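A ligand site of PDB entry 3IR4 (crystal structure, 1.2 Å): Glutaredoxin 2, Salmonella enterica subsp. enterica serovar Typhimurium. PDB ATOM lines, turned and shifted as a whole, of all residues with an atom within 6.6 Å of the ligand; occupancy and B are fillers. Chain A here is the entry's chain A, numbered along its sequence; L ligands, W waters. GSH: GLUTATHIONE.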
ATOM      1  N   TYR A   9      -6.583  18.508   3.894  1.00  0.00           N
ATOM      2  CA  TYR A   9      -5.587  19.499   4.374  1.00  0.00           C
ATOM      3  C   TYR A   9      -6.422  20.435   5.259  1.00  0.00           C
ATOM      4  O   TYR A   9      -7.500  20.874   4.862  1.00  0.00           O
ATOM      5  CB  TYR A   9      -4.945  20.296   3.253  1.00  0.00           C
ATOM      6  CG  TYR A   9      -4.268  19.475   2.192  1.00  0.00           C
ATOM      7  CD1 TYR A   9      -3.577  18.312   2.500  1.00  0.00           C
ATOM      8  CD2 TYR A   9      -4.327  19.900   0.872  1.00  0.00           C
ATOM      9  CE1 TYR A   9      -2.993  17.541   1.462  1.00  0.00           C
ATOM     10  CE2 TYR A   9      -3.746  19.152  -0.130  1.00  0.00           C
ATOM     11  CZ  TYR A   9      -3.098  17.969   0.157  1.00  0.00           C
ATOM     12  OH  TYR A   9      -2.571  17.243  -0.876  1.00  0.00           O
ATOM     13  N   HIS A  11      -6.006  23.569   6.127  1.00  0.00           N
ATOM     14  CA  HIS A  11      -6.195  24.923   5.617  1.00  0.00           C
ATOM     15  C   HIS A  11      -7.182  25.014   4.453  1.00  0.00           C
ATOM     16  O   HIS A  11      -7.640  26.091   4.109  1.00  0.00           O
ATOM     17  CB  HIS A  11      -4.864  25.505   5.093  1.00  0.00           C
ATOM     18  CG  HIS A  11      -4.485  25.043   3.716  1.00  0.00           C
ATOM     19  ND1 HIS A  11      -3.690  23.944   3.502  1.00  0.00           N
ATOM     20  CD2 HIS A  11      -4.755  25.547   2.495  1.00  0.00           C
ATOM     21  CE1 HIS A  11      -3.510  23.787   2.202  1.00  0.00           C
ATOM     22  NE2 HIS A  11      -4.162  24.745   1.565  1.00  0.00           N
ATOM     23  N   CYS A  12      -7.493  23.875   3.827  1.00  0.00           N
ATOM     24  CA  CYS A  12      -8.213  23.887   2.550  1.00  0.00           C
ATOM     25  C   CYS A  12      -9.692  24.180   2.744  1.00  0.00           C
ATOM     26  O   CYS A  12     -10.342  23.458   3.467  1.00  0.00           O
ATOM     27  CB  CYS A  12      -8.023  22.518   1.871  1.00  0.00           C
ATOM     28  SG  CYS A  12      -9.022  22.324   0.371  1.00  0.00           S
ATOM     29  N   PRO A  13     -10.217  25.246   2.108  1.00  0.00           N
ATOM     30  CA  PRO A  13     -11.615  25.554   2.305  1.00  0.00           C
ATOM     31  C   PRO A  13     -12.556  24.458   1.804  1.00  0.00           C
ATOM     32  O   PRO A  13     -13.644  24.247   2.380  1.00  0.00           O
ATOM     33  CB  PRO A  13     -11.787  26.888   1.572  1.00  0.00           C
ATOM     34  CG  PRO A  13     -10.757  26.882   0.527  1.00  0.00           C
ATOM     35  CD  PRO A  13      -9.599  26.188   1.168  1.00  0.00           C
ATOM     36  N   PHE A  14     -12.168  23.740   0.767  1.00  0.00           N
ATOM     37  CA  PHE A  14     -13.002  22.634   0.276  1.00  0.00           C
ATOM     38  C   PHE A  14     -13.104  21.529   1.316  1.00  0.00           C
ATOM     39  O   PHE A  14     -14.133  20.868   1.439  1.00  0.00           O
ATOM     40  CB  PHE A  14     -12.447  22.125  -1.061  1.00  0.00           C
ATOM     41  CG  PHE A  14     -12.414  23.160  -2.129  1.00  0.00           C
ATOM     42  CD1 PHE A  14     -11.238  23.820  -2.463  1.00  0.00           C
ATOM     43  CD2 PHE A  14     -13.577  23.568  -2.752  1.00  0.00           C
ATOM     44  CE1 PHE A  14     -11.237  24.775  -3.462  1.00  0.00           C
ATOM     45  CE2 PHE A  14     -13.563  24.547  -3.743  1.00  0.00           C
ATOM     46  CZ  PHE A  14     -12.389  25.143  -4.083  1.00  0.00           C
ATOM     47  N   CYS A  15     -12.015  21.282   2.025  1.00  0.00           N
ATOM     48  CA  CYS A  15     -12.023  20.326   3.116  1.00  0.00           C
ATOM     49  C   CYS A  15     -12.901  20.787   4.278  1.00  0.00           C
ATOM     50  O   CYS A  15     -13.632  19.990   4.878  1.00  0.00           O
ATOM     51  CB  CYS A  15     -10.599  20.072   3.581  1.00  0.00           C
ATOM     52  SG  CYS A  15      -9.634  19.153   2.331  1.00  0.00           S
ATOM     53  N   LYS A  17     -15.551  22.616   3.903  1.00  0.00           N
ATOM     54  CA  LYS A  17     -16.906  22.360   3.407  1.00  0.00           C
ATOM     55  C   LYS A  17     -17.343  20.916   3.727  1.00  0.00           C
ATOM     56  O   LYS A  17     -18.427  20.670   4.222  1.00  0.00           O
ATOM     57  CB  LYS A  17     -17.014  22.606   1.898  1.00  0.00           C
ATOM     58  CG  LYS A  17     -16.787  24.050   1.512  1.00  0.00           C
ATOM     59  CD  LYS A  17     -16.833  24.291   0.019  1.00  0.00           C
ATOM     60  CE  LYS A  17     -16.237  25.599  -0.318  1.00  0.00           C
ATOM     61  NZ  LYS A  17     -16.420  26.000  -1.722  1.00  0.00           N
ATOM     62  N   ASN A  36       1.102  17.778   2.713  1.00  0.00           N
ATOM     63  CA  ASN A  36       0.774  18.508   1.503  1.00  0.00           C
ATOM     64  C   ASN A  36       1.523  18.030   0.269  1.00  0.00           C
ATOM     65  O   ASN A  36       1.033  18.234  -0.848  1.00  0.00           O
ATOM     66  CB  ASN A  36       0.990  19.999   1.710  1.00  0.00           C
ATOM     67  CG  ASN A  36       0.281  20.865   0.677  1.00  0.00           C
ATOM     68  OD1 ASN A  36       0.938  21.541  -0.119  1.00  0.00           O
ATOM     69  ND2 ASN A  36      -1.055  20.841   0.670  1.00  0.00           N
ATOM     70  N   LYS A  49      -4.065  13.517  -6.998  1.00  0.00           N
ATOM     71  CA  LYS A  49      -3.771  14.188  -5.748  1.00  0.00           C
ATOM     72  C   LYS A  49      -4.750  15.331  -5.574  1.00  0.00           C
ATOM     73  O   LYS A  49      -4.573  16.409  -6.135  1.00  0.00           O
ATOM     74  CB  LYS A  49      -2.336  14.707  -5.786  1.00  0.00           C
ATOM     75  CG  LYS A  49      -1.908  15.405  -4.503  1.00  0.00           C
ATOM     76  CD  LYS A  49      -0.488  15.943  -4.601  1.00  0.00           C
ATOM     77  CE  LYS A  49       0.024  16.602  -3.308  1.00  0.00           C
ATOM     78  NZ  LYS A  49      -0.719  17.826  -2.950  1.00  0.00           N
ATOM     79  N   MET A  50      -5.811  15.061  -4.833  1.00  0.00           N
ATOM     80  CA  MET A  50      -6.846  16.063  -4.547  1.00  0.00           C
ATOM     81  C   MET A  50      -7.536  15.687  -3.260  1.00  0.00           C
ATOM     82  O   MET A  50      -7.728  14.499  -3.000  1.00  0.00           O
ATOM     83  CB  MET A  50      -7.860  16.162  -5.691  1.00  0.00           C
ATOM     84  CG  MET A  50      -8.856  17.307  -5.550  1.00  0.00           C
ATOM     85  SD  MET A  50     -10.040  17.538  -7.055  1.00  0.00           S
ATOM     86  CE  MET A  50     -11.092  15.943  -6.836  1.00  0.00           C
ATOM     87  N   VAL A  51      -7.858  16.707  -2.469  1.00  0.00           N
ATOM     88  CA  VAL A  51      -8.622  16.543  -1.229  1.00  0.00           C
ATOM     89  C   VAL A  51      -9.736  17.605  -1.280  1.00  0.00           C
ATOM     90  O   VAL A  51      -9.570  18.636  -1.937  1.00  0.00           O
ATOM     91  CB  VAL A  51      -7.765  16.658   0.025  1.00  0.00           C
ATOM     92  CG1 VAL A  51      -6.835  15.455   0.143  1.00  0.00           C
ATOM     93  CG2 VAL A  51      -7.021  18.006   0.070  1.00  0.00           C
ATOM     94  N   PRO A  52     -10.865  17.389  -0.595  1.00  0.00           N
ATOM     95  CA  PRO A  52     -11.164  16.278   0.317  1.00  0.00           C
ATOM     96  C   PRO A  52     -11.543  14.982  -0.378  1.00  0.00           C
ATOM     97  O   PRO A  52     -12.036  14.995  -1.515  1.00  0.00           O
ATOM     98  CB  PRO A  52     -12.406  16.777   1.061  1.00  0.00           C
ATOM     99  CG  PRO A  52     -13.068  17.729   0.098  1.00  0.00           C
ATOM    100  CD  PRO A  52     -11.914  18.436  -0.580  1.00  0.00           C
ATOM    101  N   PRO A  63     -14.644  11.796  -3.927  1.00  0.00           N
ATOM    102  CA  PRO A  63     -14.071  13.139  -3.924  1.00  0.00           C
ATOM    103  C   PRO A  63     -15.172  14.173  -4.220  1.00  0.00           C
ATOM    104  O   PRO A  63     -16.327  13.818  -4.449  1.00  0.00           O
ATOM    105  CB  PRO A  63     -13.072  13.062  -5.086  1.00  0.00           C
ATOM    106  CG  PRO A  63     -13.759  12.164  -6.046  1.00  0.00           C
ATOM    107  CD  PRO A  63     -14.559  11.182  -5.253  1.00  0.00           C
ATOM    108  N   GLU A  64     -14.756  15.430  -4.259  1.00  0.00           N
ATOM    109  CA  GLU A  64     -15.546  16.634  -4.557  1.00  0.00           C
ATOM    110  C   GLU A  64     -16.352  17.110  -3.352  1.00  0.00           C
ATOM    111  O   GLU A  64     -17.338  16.490  -2.964  1.00  0.00           O
ATOM    112  CB  GLU A  64     -16.462  16.481  -5.776  1.00  0.00           C
ATOM    113  CG  GLU A  64     -15.716  16.185  -7.056  1.00  0.00           C
ATOM    114  CD  GLU A  64     -14.887  17.349  -7.559  1.00  0.00           C
ATOM    115  OE1 GLU A  64     -15.097  18.505  -7.115  1.00  0.00           O
ATOM    116  OE2 GLU A  64     -14.047  17.064  -8.461  1.00  0.00           O
ATOM    117  N   SER A  65     -15.900  18.216  -2.802  1.00  0.00           N
ATOM    118  CA  SER A  65     -16.526  18.777  -1.615  1.00  0.00           C
ATOM    119  C   SER A  65     -18.038  18.815  -1.627  1.00  0.00           C
ATOM    120  O   SER A  65     -18.664  18.360  -0.665  1.00  0.00           O
ATOM    121  CB  SER A  65     -15.973  20.178  -1.319  1.00  0.00           C
ATOM    122  OG  SER A  65     -16.201  21.048  -2.377  1.00  0.00           O
ATOM    123  N   MET A  66     -18.631  19.306  -2.692  1.00  0.00           N
ATOM    124  CA  MET A  66     -20.109  19.455  -2.670  1.00  0.00           C
ATOM    125  C   MET A  66     -20.802  18.101  -2.804  1.00  0.00           C
ATOM    126  O   MET A  66     -21.909  17.933  -2.302  1.00  0.00           O
ATOM    127  CB  MET A  66     -20.571  20.456  -3.701  1.00  0.00           C
ATOM    128  CG  MET A  66     -20.069  21.870  -3.491  1.00  0.00           C
ATOM    129  SD  MET A  66     -20.261  22.566  -1.677  1.00  0.00           S
ATOM    130  CE  MET A  66     -22.173  22.490  -1.537  1.00  0.00           C
ATOM    131  N   ILE A  68     -19.623  15.343  -1.473  1.00  0.00           N
ATOM    132  CA  ILE A  68     -19.517  14.840  -0.115  1.00  0.00           C
ATOM    133  C   ILE A  68     -20.598  15.504   0.754  1.00  0.00           C
ATOM    134  O   ILE A  68     -21.269  14.832   1.508  1.00  0.00           O
ATOM    135  CB  ILE A  68     -18.102  15.101   0.443  1.00  0.00           C
ATOM    136  CG1 ILE A  68     -17.062  14.310  -0.350  1.00  0.00           C
ATOM    137  CG2 ILE A  68     -18.033  14.781   1.938  1.00  0.00           C
ATOM    138  CD1 ILE A  68     -15.643  14.740  -0.060  1.00  0.00           C
ATOM    139  N   TYR A 124       7.069  22.465  -0.458  1.00  0.00           N
ATOM    140  CA  TYR A 124       6.253  22.058  -1.596  1.00  0.00           C
ATOM    141  C   TYR A 124       5.108  23.052  -1.825  1.00  0.00           C
ATOM    142  O   TYR A 124       4.857  23.497  -2.945  1.00  0.00           O
ATOM    143  CB  TYR A 124       5.702  20.656  -1.351  1.00  0.00           C
ATOM    144  CG  TYR A 124       4.769  20.161  -2.412  1.00  0.00           C
ATOM    145  CD1 TYR A 124       3.401  20.394  -2.315  1.00  0.00           C
ATOM    146  CD2 TYR A 124       5.207  19.387  -3.458  1.00  0.00           C
ATOM    147  CE1 TYR A 124       2.513  19.918  -3.251  1.00  0.00           C
ATOM    148  CE2 TYR A 124       4.327  18.942  -4.427  1.00  0.00           C
ATOM    149  CZ  TYR A 124       2.965  19.218  -4.317  1.00  0.00           C
ATOM    150  OH  TYR A 124       2.010  18.765  -5.214  1.00  0.00           O
ATOM    151  N   LYS A 128       4.814  25.800  -5.031  1.00  0.00           N
ATOM    152  CA  LYS A 128       3.683  25.667  -5.938  1.00  0.00           C
ATOM    153  C   LYS A 128       2.868  26.952  -6.010  1.00  0.00           C
ATOM    154  O   LYS A 128       2.514  27.397  -7.090  1.00  0.00           O
ATOM    155  CB  LYS A 128       2.797  24.532  -5.454  1.00  0.00           C
ATOM    156  CG  LYS A 128       1.557  24.356  -6.281  1.00  0.00           C
ATOM    157  CD  LYS A 128       0.622  23.385  -5.687  1.00  0.00           C
ATOM    158  CE  LYS A 128       1.136  22.035  -5.824  1.00  0.00           C
ATOM    159  NZ  LYS A 128       0.103  21.149  -5.230  1.00  0.00           N
ATOM    160  N   LYS A 129       2.570  27.547  -4.869  1.00  0.00           N
ATOM    161  CA  LYS A 129       1.740  28.739  -4.884  1.00  0.00           C
ATOM    162  C   LYS A 129       2.502  29.929  -5.461  1.00  0.00           C
ATOM    163  O   LYS A 129       1.942  30.704  -6.250  1.00  0.00           O
ATOM    164  CB  LYS A 129       1.227  29.065  -3.486  1.00  0.00           C
ATOM    165  CG  LYS A 129       0.330  27.968  -2.901  1.00  0.00           C
ATOM    166  CD  LYS A 129      -0.887  27.638  -3.775  1.00  0.00           C
ATOM    167  CE  LYS A 129      -1.769  26.615  -3.158  1.00  0.00           C
ATOM    168  NZ  LYS A 129      -2.866  26.243  -4.102  1.00  0.00           N
HETATM  169  N1  GSH L   1     -13.365  20.652  -6.860  1.00  0.00           N
HETATM  170  CA1 GSH L   1     -12.666  20.176  -5.654  1.00  0.00           C
HETATM  171  C1  GSH L   1     -13.643  20.051  -4.522  1.00  0.00           C
HETATM  172  O11 GSH L   1     -14.668  20.793  -4.552  1.00  0.00           O
HETATM  173  O12 GSH L   1     -13.391  19.261  -3.596  1.00  0.00           O
HETATM  174  CB1 GSH L   1     -11.554  21.163  -5.328  1.00  0.00           C
HETATM  175  CG1 GSH L   1     -10.610  20.595  -4.263  1.00  0.00           C
HETATM  176  CD1 GSH L   1      -9.292  21.313  -4.159  1.00  0.00           C
HETATM  177  OE1 GSH L   1      -9.053  22.409  -4.905  1.00  0.00           O
HETATM  178  N2  GSH L   1      -8.408  20.897  -3.290  1.00  0.00           N
HETATM  179  CA2 GSH L   1      -7.022  21.364  -3.213  1.00  0.00           C
HETATM  180  C2  GSH L   1      -6.095  20.299  -3.674  1.00  0.00           C
HETATM  181  O2  GSH L   1      -6.362  19.027  -3.393  1.00  0.00           O
HETATM  182  CB2 GSH L   1      -6.668  21.806  -1.766  1.00  0.00           C
HETATM  183  SG2 GSH L   1      -7.581  23.244  -1.123  1.00  0.00           S
HETATM  184  N3  GSH L   1      -5.002  20.643  -4.309  1.00  0.00           N
HETATM  185  CA3 GSH L   1      -4.192  19.683  -5.026  1.00  0.00           C
HETATM  186  C3  GSH L   1      -2.846  19.627  -4.404  1.00  0.00           C
HETATM  187  O31 GSH L   1      -2.688  20.147  -3.261  1.00  0.00           O
HETATM  188  O32 GSH L   1      -1.930  19.050  -5.040  1.00  0.00           O
HETATM  189  O   HOH W   1      -5.902  18.470  -7.562  1.00  0.00           O
HETATM  190  O   HOH W   2      -2.898  22.618  -1.121  1.00  0.00           O
HETATM  191  O   HOH W   3      -0.497  21.022  -2.598  1.00  0.00           O
HETATM  192  O   HOH W   4      -7.724  24.876  -4.364  1.00  0.00           O
HETATM  193  O   HOH W   5      -3.276  23.023  -6.126  1.00  0.00           O
HETATM  194  O   HOH W   6      -7.519  20.525  -6.778  1.00  0.00           O
HETATM  195  O   HOH W   7      -2.265  18.080  -7.382  1.00  0.00           O
HETATM  196  O   HOH W   8      -5.037  24.353  -3.509  1.00  0.00           O
HETATM  197  O   HOH W   9     -14.941  23.023  -7.143  1.00  0.00           O
HETATM  198  O   HOH W  10      -2.481  23.170  -3.560  1.00  0.00           O
HETATM  199  O   HOH W  11     -12.223  16.658  -3.703  1.00  0.00           O
HETATM  200  O   HOH W  12     -17.493  20.131  -5.328  1.00  0.00           O
HETATM  201  O   HOH W  13     -10.074  23.994  -6.879  1.00  0.00           O
HETATM  202  O   HOH W  14     -11.575  20.875  -9.005  1.00  0.00           O
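SG of Cys 12 is covalently linked to SG2 of the ligand (2.3 Å). The backbone NH (N) of Ser 65 lies within hydrogen-bond range of an oxygen (O12) of the ligand. OG of Ser 65 sits at hydrogen-bond distance from O11 of the ligand (2.7 Å). An oxygen (O32) of the ligand lies within salt-bridge range of the side-chain amino group (NZ) of Lys 49, 2.7 Å away. OE1 of Glu 64 lies within salt-bridge range of N1 of the ligand (2.8 Å). The backbone NH (N) of Val 51 is in hydrogen-bond range of an oxygen (O2) of the ligand, at 2.9 Å. The backbone carbonyl oxygen of Val 51 lies within hydrogen-bond range of a nitrogen (N2) of the ligand, 2.9 Å away. NZ of Lys 128 lies within salt-bridge range of O32 of the ligand (2.9 Å).
SG of Cys 12 sits close to N of Phe 14 (3.5 Å). The side-chain sulfur (SG) of Cys 12 sits at hydrogen-bond distance from the backbone NH (N) of Cys 15 (3.6 Å). The side-chain hydroxyl (OH) of Tyr 9 is in hydrogen-bond range of the side-chain amino group (NZ) of Lys 49 (2.8 Å). NZ of Lys 49 is in hydrogen-bond range of O of Asn 36, 2.8 Å away. NZ of Lys 128 lies within hydrogen-bond range of OH of Tyr 124, at 3.1 Å. The backbone NH (N) of Tyr 9 sits at hydrogen-bond distance from the side-chain sulfur (SG) of Cys 15, at 3.5 Å.
Merely in contact with the ligand: Met 50, Tyr 9, Pro 52, Phe 14 and Tyr 124. The nearest printed residue that does not touch the ligand is Pro 13 (4.2 Å).
Water W3 lies within hydrogen-bond range of an oxygen (O31) of the ligand, the side-chain amino group of Lys 128, the side-chain amide oxygen of Asn 36 and the side-chain amino group of Lys 49. Water W11 lies within hydrogen-bond range of the backbone carbonyl oxygen (O) of Pro 52 (2.8 Å), an oxygen (O12) of the ligand (2.9 Å) and the backbone NH (N) of Glu 64 (2.9 Å). Water W12 lies within hydrogen-bond range of N of Met 66, O11 of the ligand, OG of Ser 65 and OE1 of Glu 64. Water W10 bridges O31 of the ligand (3.0 Å) and NZ of Lys 129 (3.1 Å). Water W2 bridges the side-chain amide nitrogen of Asn 36 (3.1 Å) and an oxygen (O31) of the ligand (3.3 Å). Water W8 bridges NZ of Lys 129 and SG2 of the ligand.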
